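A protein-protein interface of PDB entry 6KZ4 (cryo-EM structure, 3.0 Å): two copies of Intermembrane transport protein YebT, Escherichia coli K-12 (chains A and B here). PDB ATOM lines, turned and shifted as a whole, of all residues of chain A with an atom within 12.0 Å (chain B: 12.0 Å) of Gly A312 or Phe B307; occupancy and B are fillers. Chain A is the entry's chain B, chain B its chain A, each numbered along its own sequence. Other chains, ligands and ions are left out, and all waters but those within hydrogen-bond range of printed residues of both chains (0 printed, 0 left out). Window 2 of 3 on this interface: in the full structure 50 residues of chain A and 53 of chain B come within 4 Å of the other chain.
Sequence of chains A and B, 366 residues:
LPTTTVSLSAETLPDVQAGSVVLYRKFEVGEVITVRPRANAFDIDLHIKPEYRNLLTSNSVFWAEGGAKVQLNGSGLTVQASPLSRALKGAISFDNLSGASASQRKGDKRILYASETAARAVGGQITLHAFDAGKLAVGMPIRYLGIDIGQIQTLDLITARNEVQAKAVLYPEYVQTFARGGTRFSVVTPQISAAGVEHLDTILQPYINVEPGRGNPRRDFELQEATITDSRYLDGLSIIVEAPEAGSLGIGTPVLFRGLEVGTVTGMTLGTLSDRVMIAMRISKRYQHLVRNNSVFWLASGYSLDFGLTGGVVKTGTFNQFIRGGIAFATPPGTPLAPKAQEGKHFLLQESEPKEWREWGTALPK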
ATOM      1  N   SER A 304     -27.543  -0.713   6.449  1.00  0.00           N
ATOM      2  CA  SER A 304     -28.420  -0.240   5.378  1.00  0.00           C
ATOM      3  C   SER A 304     -28.643   1.255   5.579  1.00  0.00           C
ATOM      4  O   SER A 304     -29.521   1.660   6.345  1.00  0.00           O
ATOM      5  CB  SER A 304     -29.740  -1.005   5.377  1.00  0.00           C
ATOM      6  OG  SER A 304     -30.761  -0.260   4.736  1.00  0.00           O
ATOM      7  N   LEU A 305     -27.858   2.071   4.885  1.00  0.00           N
ATOM      8  CA  LEU A 305     -27.874   3.508   5.112  1.00  0.00           C
ATOM      9  C   LEU A 305     -29.103   4.155   4.482  1.00  0.00           C
ATOM     10  O   LEU A 305     -29.645   3.677   3.482  1.00  0.00           O
ATOM     11  CB  LEU A 305     -26.604   4.149   4.555  1.00  0.00           C
ATOM     12  CG  LEU A 305     -25.316   3.941   5.354  1.00  0.00           C
ATOM     13  CD1 LEU A 305     -24.635   2.630   4.991  1.00  0.00           C
ATOM     14  CD2 LEU A 305     -24.368   5.109   5.150  1.00  0.00           C
ATOM     15  N   ASP A 306     -29.541   5.256   5.087  1.00  0.00           N
ATOM     16  CA  ASP A 306     -30.678   6.020   4.601  1.00  0.00           C
ATOM     17  C   ASP A 306     -30.253   6.941   3.460  1.00  0.00           C
ATOM     18  O   ASP A 306     -29.085   6.994   3.071  1.00  0.00           O
ATOM     19  CB  ASP A 306     -31.291   6.845   5.732  1.00  0.00           C
ATOM     20  CG  ASP A 306     -31.704   6.000   6.915  1.00  0.00           C
ATOM     21  OD1 ASP A 306     -32.262   4.905   6.692  1.00  0.00           O
ATOM     22  OD2 ASP A 306     -31.475   6.427   8.066  1.00  0.00           O
ATOM     23  N   PHE A 307     -31.225   7.677   2.923  1.00  0.00           N
ATOM     24  CA  PHE A 307     -30.936   8.734   1.955  1.00  0.00           C
ATOM     25  C   PHE A 307     -32.151   9.645   1.880  1.00  0.00           C
ATOM     26  O   PHE A 307     -33.226   9.206   1.457  1.00  0.00           O
ATOM     27  CB  PHE A 307     -30.600   8.146   0.582  1.00  0.00           C
ATOM     28  CG  PHE A 307     -30.056   9.150  -0.392  1.00  0.00           C
ATOM     29  CD1 PHE A 307     -28.750   9.602  -0.277  1.00  0.00           C
ATOM     30  CD2 PHE A 307     -30.843   9.639  -1.421  1.00  0.00           C
ATOM     31  CE1 PHE A 307     -28.238  10.525  -1.168  1.00  0.00           C
ATOM     32  CE2 PHE A 307     -30.340  10.561  -2.318  1.00  0.00           C
ATOM     33  CZ  PHE A 307     -29.034  11.007  -2.191  1.00  0.00           C
ATOM     34  N   GLY A 308     -31.987  10.898   2.284  1.00  0.00           N
ATOM     35  CA  GLY A 308     -33.098  11.827   2.353  1.00  0.00           C
ATOM     36  C   GLY A 308     -32.919  12.990   1.401  1.00  0.00           C
ATOM     37  O   GLY A 308     -31.810  13.307   0.971  1.00  0.00           O
ATOM     38  N   LEU A 309     -34.045  13.626   1.070  1.00  0.00           N
ATOM     39  CA  LEU A 309     -34.030  14.714   0.095  1.00  0.00           C
ATOM     40  C   LEU A 309     -33.632  16.036   0.742  1.00  0.00           C
ATOM     41  O   LEU A 309     -32.597  16.621   0.405  1.00  0.00           O
ATOM     42  CB  LEU A 309     -35.405  14.850  -0.566  1.00  0.00           C
ATOM     43  CG  LEU A 309     -35.739  13.956  -1.763  1.00  0.00           C
ATOM     44  CD1 LEU A 309     -34.783  14.208  -2.924  1.00  0.00           C
ATOM     45  CD2 LEU A 309     -35.771  12.488  -1.368  1.00  0.00           C
ATOM     46  N   THR A 310     -34.450  16.523   1.678  1.00  0.00           N
ATOM     47  CA  THR A 310     -34.175  17.809   2.309  1.00  0.00           C
ATOM     48  C   THR A 310     -33.355  17.634   3.580  1.00  0.00           C
ATOM     49  O   THR A 310     -32.383  18.362   3.807  1.00  0.00           O
ATOM     50  CB  THR A 310     -35.485  18.534   2.615  1.00  0.00           C
ATOM     51  OG1 THR A 310     -36.295  17.715   3.468  1.00  0.00           O
ATOM     52  CG2 THR A 310     -36.246  18.821   1.328  1.00  0.00           C
ATOM     53  N   GLY A 311     -33.735  16.678   4.420  1.00  0.00           N
ATOM     54  CA  GLY A 311     -32.940  16.326   5.577  1.00  0.00           C
ATOM     55  C   GLY A 311     -32.885  14.825   5.742  1.00  0.00           C
ATOM     56  O   GLY A 311     -33.918  14.173   5.919  1.00  0.00           O
ATOM     57  N   GLY A 312     -31.683  14.263   5.682  1.00  0.00           N
ATOM     58  CA  GLY A 312     -31.530  12.827   5.782  1.00  0.00           C
ATOM     59  C   GLY A 312     -30.378  12.429   6.675  1.00  0.00           C
ATOM     60  O   GLY A 312     -29.226  12.783   6.411  1.00  0.00           O
ATOM     61  N   VAL A 313     -30.673  11.696   7.726  1.00  0.00           N
ATOM     62  CA  VAL A 313     -29.653  11.225   8.652  1.00  0.00           C
ATOM     63  C   VAL A 313     -29.269   9.809   8.262  1.00  0.00           C
ATOM     64  O   VAL A 313     -30.124   8.997   7.893  1.00  0.00           O
ATOM     65  CB  VAL A 313     -30.162  11.290  10.104  1.00  0.00           C
ATOM     66  CG1 VAL A 313     -29.003  11.174  11.081  1.00  0.00           C
ATOM     67  CG2 VAL A 313     -30.940  12.576  10.335  1.00  0.00           C
ATOM     68  N   VAL A 314     -27.976   9.510   8.328  1.00  0.00           N
ATOM     69  CA  VAL A 314     -27.470   8.171   8.061  1.00  0.00           C
ATOM     70  C   VAL A 314     -27.073   7.535   9.384  1.00  0.00           C
ATOM     71  O   VAL A 314     -26.586   8.215  10.298  1.00  0.00           O
ATOM     72  CB  VAL A 314     -26.297   8.185   7.061  1.00  0.00           C
ATOM     73  CG1 VAL A 314     -26.678   8.970   5.815  1.00  0.00           C
ATOM     74  CG2 VAL A 314     -25.052   8.768   7.691  1.00  0.00           C
ATOM     75  N   LYS A 315     -27.312   6.233   9.497  1.00  0.00           N
ATOM     76  CA  LYS A 315     -27.078   5.481  10.717  1.00  0.00           C
ATOM     77  C   LYS A 315     -26.065   4.381  10.445  1.00  0.00           C
ATOM     78  O   LYS A 315     -25.996   3.852   9.330  1.00  0.00           O
ATOM     79  CB  LYS A 315     -28.382   4.875  11.245  1.00  0.00           C
ATOM     80  CG  LYS A 315     -29.103   3.972  10.243  1.00  0.00           C
ATOM     81  CD  LYS A 315     -28.818   2.502  10.512  1.00  0.00           C
ATOM     82  CE  LYS A 315     -29.526   1.605   9.521  1.00  0.00           C
ATOM     83  NZ  LYS A 315     -29.152   0.177   9.717  1.00  0.00           N
ATOM     84  N   THR A 316     -25.287   4.033  11.457  1.00  0.00           N
ATOM     85  CA  THR A 316     -24.325   2.952  11.315  1.00  0.00           C
ATOM     86  C   THR A 316     -24.459   1.879  12.383  1.00  0.00           C
ATOM     87  O   THR A 316     -24.303   0.696  12.076  1.00  0.00           O
ATOM     88  CB  THR A 316     -22.893   3.510  11.318  1.00  0.00           C
ATOM     89  OG1 THR A 316     -21.956   2.427  11.329  1.00  0.00           O
ATOM     90  CG2 THR A 316     -22.660   4.399  12.523  1.00  0.00           C
ATOM     91  N   TYR B 303     -22.119   6.371  15.224  1.00  0.00           N
ATOM     92  CA  TYR B 303     -22.047   7.687  14.615  1.00  0.00           C
ATOM     93  C   TYR B 303     -23.362   8.029  13.931  1.00  0.00           C
ATOM     94  O   TYR B 303     -24.104   7.148  13.490  1.00  0.00           O
ATOM     95  CB  TYR B 303     -20.903   7.755  13.604  1.00  0.00           C
ATOM     96  CG  TYR B 303     -19.615   7.144  14.099  1.00  0.00           C
ATOM     97  CD1 TYR B 303     -18.812   7.813  15.009  1.00  0.00           C
ATOM     98  CD2 TYR B 303     -19.196   5.902  13.647  1.00  0.00           C
ATOM     99  CE1 TYR B 303     -17.631   7.260  15.461  1.00  0.00           C
ATOM    100  CE2 TYR B 303     -18.016   5.342  14.093  1.00  0.00           C
ATOM    101  CZ  TYR B 303     -17.239   6.024  14.999  1.00  0.00           C
ATOM    102  OH  TYR B 303     -16.063   5.470  15.446  1.00  0.00           O
ATOM    103  N   SER B 304     -23.648   9.327  13.854  1.00  0.00           N
ATOM    104  CA  SER B 304     -24.815   9.853  13.145  1.00  0.00           C
ATOM    105  C   SER B 304     -24.315  11.002  12.277  1.00  0.00           C
ATOM    106  O   SER B 304     -24.346  12.163  12.691  1.00  0.00           O
ATOM    107  CB  SER B 304     -25.901  10.304  14.115  1.00  0.00           C
ATOM    108  OG  SER B 304     -26.713   9.216  14.520  1.00  0.00           O
ATOM    109  N   LEU B 305     -23.869  10.678  11.069  1.00  0.00           N
ATOM    110  CA  LEU B 305     -23.287  11.681  10.194  1.00  0.00           C
ATOM    111  C   LEU B 305     -24.365  12.594   9.624  1.00  0.00           C
ATOM    112  O   LEU B 305     -25.505  12.180   9.396  1.00  0.00           O
ATOM    113  CB  LEU B 305     -22.494  11.017   9.069  1.00  0.00           C
ATOM    114  CG  LEU B 305     -21.444   9.994   9.516  1.00  0.00           C
ATOM    115  CD1 LEU B 305     -21.985   8.571   9.494  1.00  0.00           C
ATOM    116  CD2 LEU B 305     -20.188  10.109   8.666  1.00  0.00           C
ATOM    117  N   ASP B 306     -23.988  13.849   9.396  1.00  0.00           N
ATOM    118  CA  ASP B 306     -24.925  14.894   9.021  1.00  0.00           C
ATOM    119  C   ASP B 306     -25.142  14.917   7.510  1.00  0.00           C
ATOM    120  O   ASP B 306     -24.592  14.107   6.759  1.00  0.00           O
ATOM    121  CB  ASP B 306     -24.425  16.251   9.510  1.00  0.00           C
ATOM    122  CG  ASP B 306     -24.299  16.315  11.013  1.00  0.00           C
ATOM    123  OD1 ASP B 306     -25.027  15.571  11.701  1.00  0.00           O
ATOM    124  OD2 ASP B 306     -23.470  17.109  11.509  1.00  0.00           O
ATOM    125  N   PHE B 307     -25.955  15.870   7.058  1.00  0.00           N
ATOM    126  CA  PHE B 307     -26.304  15.994   5.652  1.00  0.00           C
ATOM    127  C   PHE B 307     -26.775  17.414   5.379  1.00  0.00           C
ATOM    128  O   PHE B 307     -27.552  17.978   6.155  1.00  0.00           O
ATOM    129  CB  PHE B 307     -27.394  14.993   5.259  1.00  0.00           C
ATOM    130  CG  PHE B 307     -27.430  14.676   3.792  1.00  0.00           C
ATOM    131  CD1 PHE B 307     -26.703  13.613   3.283  1.00  0.00           C
ATOM    132  CD2 PHE B 307     -28.197  15.435   2.925  1.00  0.00           C
ATOM    133  CE1 PHE B 307     -26.735  13.316   1.932  1.00  0.00           C
ATOM    134  CE2 PHE B 307     -28.235  15.144   1.573  1.00  0.00           C
ATOM    135  CZ  PHE B 307     -27.502  14.083   1.077  1.00  0.00           C
ATOM    136  N   GLY B 308     -26.302  17.980   4.280  1.00  0.00           N
ATOM    137  CA  GLY B 308     -26.694  19.323   3.890  1.00  0.00           C
ATOM    138  C   GLY B 308     -26.666  19.465   2.387  1.00  0.00           C
ATOM    139  O   GLY B 308     -25.763  18.957   1.713  1.00  0.00           O
ATOM    140  N   LEU B 309     -27.667  20.170   1.856  1.00  0.00           N
ATOM    141  CA  LEU B 309     -27.779  20.335   0.410  1.00  0.00           C
ATOM    142  C   LEU B 309     -26.730  21.310  -0.114  1.00  0.00           C
ATOM    143  O   LEU B 309     -25.867  20.938  -0.915  1.00  0.00           O
ATOM    144  CB  LEU B 309     -29.189  20.804   0.037  1.00  0.00           C
ATOM    145  CG  LEU B 309     -30.313  19.766  -0.074  1.00  0.00           C
ATOM    146  CD1 LEU B 309     -30.059  18.815  -1.236  1.00  0.00           C
ATOM    147  CD2 LEU B 309     -30.525  18.992   1.222  1.00  0.00           C
ATOM    148  N   THR B 310     -26.789  22.566   0.332  1.00  0.00           N
ATOM    149  CA  THR B 310     -25.749  23.516  -0.046  1.00  0.00           C
ATOM    150  C   THR B 310     -24.424  23.195   0.635  1.00  0.00           C
ATOM    151  O   THR B 310     -23.369  23.295   0.002  1.00  0.00           O
ATOM    152  CB  THR B 310     -26.196  24.953   0.260  1.00  0.00           C
ATOM    153  OG1 THR B 310     -25.261  25.880  -0.306  1.00  0.00           O
ATOM    154  CG2 THR B 310     -26.330  25.206   1.761  1.00  0.00           C
ATOM    155  N   GLY B 311     -24.456  22.785   1.899  1.00  0.00           N
ATOM    156  CA  GLY B 311     -23.260  22.345   2.585  1.00  0.00           C
ATOM    157  C   GLY B 311     -23.578  21.711   3.920  1.00  0.00           C
ATOM    158  O   GLY B 311     -24.285  22.300   4.745  1.00  0.00           O
ATOM    159  N   GLY B 312     -23.053  20.513   4.151  1.00  0.00           N
ATOM    160  CA  GLY B 312     -23.262  19.839   5.413  1.00  0.00           C
ATOM    161  C   GLY B 312     -21.966  19.336   6.006  1.00  0.00           C
ATOM    162  O   GLY B 312     -21.316  18.451   5.441  1.00  0.00           O
ATOM    163  N   VAL B 313     -21.580  19.894   7.152  1.00  0.00           N
ATOM    164  CA  VAL B 313     -20.376  19.436   7.828  1.00  0.00           C
ATOM    165  C   VAL B 313     -20.661  18.090   8.475  1.00  0.00           C
ATOM    166  O   VAL B 313     -21.749  17.858   9.017  1.00  0.00           O
ATOM    167  CB  VAL B 313     -19.919  20.476   8.864  1.00  0.00           C
ATOM    168  CG1 VAL B 313     -18.659  20.009   9.579  1.00  0.00           C
ATOM    169  CG2 VAL B 313     -19.704  21.826   8.202  1.00  0.00           C
ATOM    170  N   VAL B 314     -19.687  17.188   8.416  1.00  0.00           N
ATOM    171  CA  VAL B 314     -19.833  15.844   8.959  1.00  0.00           C
ATOM    172  C   VAL B 314     -18.930  15.706  10.176  1.00  0.00           C
ATOM    173  O   VAL B 314     -17.868  16.336  10.257  1.00  0.00           O
ATOM    174  CB  VAL B 314     -19.517  14.771   7.899  1.00  0.00           C
ATOM    175  CG1 VAL B 314     -20.321  15.033   6.639  1.00  0.00           C
ATOM    176  CG2 VAL B 314     -18.042  14.754   7.585  1.00  0.00           C
ATOM    177  N   LYS B 315     -19.365  14.889  11.132  1.00  0.00           N
ATOM    178  CA  LYS B 315     -18.670  14.702  12.397  1.00  0.00           C
ATOM    179  C   LYS B 315     -18.285  13.238  12.536  1.00  0.00           C
ATOM    180  O   LYS B 315     -19.061  12.351  12.166  1.00  0.00           O
ATOM    181  CB  LYS B 315     -19.547  15.147  13.576  1.00  0.00           C
ATOM    182  CG  LYS B 315     -20.877  14.404  13.704  1.00  0.00           C
ATOM    183  CD  LYS B 315     -20.799  13.313  14.765  1.00  0.00           C
ATOM    184  CE  LYS B 315     -22.113  12.578  14.915  1.00  0.00           C
ATOM    185  NZ  LYS B 315     -22.004  11.472  15.905  1.00  0.00           N
ATOM    186  N   THR B 316     -17.084  12.985  13.048  1.00  0.00           N
ATOM    187  CA  THR B 316     -16.615  11.620  13.223  1.00  0.00           C
ATOM    188  C   THR B 316     -16.401  11.246  14.680  1.00  0.00           C
ATOM    189  O   THR B 316     -17.025  10.298  15.166  1.00  0.00           O
ATOM    190  CB  THR B 316     -15.313  11.409  12.439  1.00  0.00           C
ATOM    191  OG1 THR B 316     -15.428  12.024  11.153  1.00  0.00           O
ATOM    192  CG2 THR B 316     -15.045   9.929  12.256  1.00  0.00           C
ATOM    193  N   GLU B 351     -35.847   8.687  20.277  1.00  0.00           N
ATOM    194  CA  GLU B 351     -34.902   8.406  19.202  1.00  0.00           C
ATOM    195  C   GLU B 351     -34.405   9.654  18.484  1.00  0.00           C
ATOM    196  O   GLU B 351     -33.649   9.520  17.517  1.00  0.00           O
ATOM    197  CB  GLU B 351     -35.554   7.470  18.187  1.00  0.00           C
ATOM    198  CG  GLU B 351     -36.595   8.147  17.302  1.00  0.00           C
ATOM    199  CD  GLU B 351     -37.950   8.302  17.974  1.00  0.00           C
ATOM    200  OE1 GLU B 351     -38.011   8.340  19.221  1.00  0.00           O
ATOM    201  OE2 GLU B 351     -38.965   8.382  17.249  1.00  0.00           O
ATOM    202  N   SER B 352     -34.793  10.849  18.918  1.00  0.00           N
ATOM    203  CA  SER B 352     -34.577  12.050  18.126  1.00  0.00           C
ATOM    204  C   SER B 352     -33.331  12.836  18.511  1.00  0.00           C
ATOM    205  O   SER B 352     -32.874  13.649  17.701  1.00  0.00           O
ATOM    206  CB  SER B 352     -35.801  12.971  18.224  1.00  0.00           C
ATOM    207  OG  SER B 352     -37.005  12.238  18.073  1.00  0.00           O
ATOM    208  N   GLU B 353     -32.759  12.606  19.701  1.00  0.00           N
ATOM    209  CA  GLU B 353     -31.650  13.423  20.187  1.00  0.00           C
ATOM    210  C   GLU B 353     -32.027  14.899  20.153  1.00  0.00           C
ATOM    211  O   GLU B 353     -31.665  15.601  19.202  1.00  0.00           O
ATOM    212  CB  GLU B 353     -30.375  13.192  19.376  1.00  0.00           C
ATOM    213  CG  GLU B 353     -29.196  14.017  19.873  1.00  0.00           C
ATOM    214  CD  GLU B 353     -28.016  13.989  18.932  1.00  0.00           C
ATOM    215  OE1 GLU B 353     -27.973  13.103  18.054  1.00  0.00           O
ATOM    216  OE2 GLU B 353     -27.129  14.857  19.071  1.00  0.00           O
ATOM    217  N   LYS B 355     -32.591  18.483  19.532  1.00  0.00           N
ATOM    218  CA  LYS B 355     -31.585  19.286  18.846  1.00  0.00           C
ATOM    219  C   LYS B 355     -31.099  20.450  19.699  1.00  0.00           C
ATOM    220  O   LYS B 355     -29.943  20.868  19.572  1.00  0.00           O
ATOM    221  CB  LYS B 355     -32.147  19.788  17.517  1.00  0.00           C
ATOM    222  CG  LYS B 355     -33.421  20.601  17.651  1.00  0.00           C
ATOM    223  CD  LYS B 355     -33.696  21.417  16.399  1.00  0.00           C
ATOM    224  CE  LYS B 355     -33.681  20.540  15.158  1.00  0.00           C
ATOM    225  NZ  LYS B 355     -34.554  21.084  14.082  1.00  0.00           N
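Among the printed residues, merely in contact across the chains: Leu A309 with Leu B309 (3.3 Å), Thr A310 with Leu B309 (3.2 Å), Gly A312 with Phe B307 (3.1 Å), Val A314 with Ser B304 (3.7 Å), Val A314 with Leu B305 (3.6 Å) and Thr A316 with Tyr B303 (3.3 Å).
No residue of chain B comes within 4 Å of Asp A306. Phe A307 touches none of the printed residues of chain B. No residue of chain B comes within 4 Å of Gly A308. Of the printed residues of chain B, Leu A309 touches Leu B309. Printed residues of chain B within 4 Å of Thr A310: Leu B309 (3.2 Å). Gly A311 touches none of the printed residues of chain B. Gly A312 touches just one residue of chain B: Phe B307 (3.1 Å). Printed residues of chain B within 4 Å of Val A314: Ser B304 and Leu B305. Lys A315 touches none of the printed residues of chain B. Of the printed residues of chain B, Thr A316 touches Tyr B303 (3.3 Å). Of the printed residues of chain A, Tyr B303 touches Thr A316 (3.3 Å). Of the printed residues of chain A, Leu B305 touches Val A314 (3.6 Å). Phe B307 touches just one residue of chain A: Gly A312 (3.1 Å). No residue of chain A comes within 4 Å of Gly B308. Of chain A, only Leu A309 and Thr A310 come within 4 Å of Leu B309. No residue of chain A comes within 4 Å of Gly B312. Val B313 touches none of the printed residues of chain A. The nearest residue of chain A that does not touch Phe B307 is Gly A308 (4.1 Å). The nearest printed residue of chain B that does not touch Leu A309 is Phe B307 (4.8 Å).
Hydrophobic or aromatic side chains of chain B within 4 Å of the printed part of chain A: Tyr B303, Leu B305, Phe B307 and Leu B309. Among the printed residues, 6 pairs touch across the chains.
Thr A310 touches Leu B309, but with the chains exchanged Leu A309 does not touch Thr B310 (8.3 Å). Gly A312 touches Phe B307, but with the chains exchanged Phe A307 does not touch Gly B312 (12.4 Å). Val A314 touches Ser B304, but with the chains exchanged Ser A304 does not touch Val B314 (16.1 Å). Val A314 touches Leu B305, but with the chains exchanged Leu A305 does not touch Val B314 (10.8 Å). Positions printed for both chains: 304, 305, 306, 307, 308, 309, 310, 311, 312, 313, 314, 315 and 316. Of the 6 pairs that touch across the chains among the printed residues, 1 has its exchanged pair printed and touching as well.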
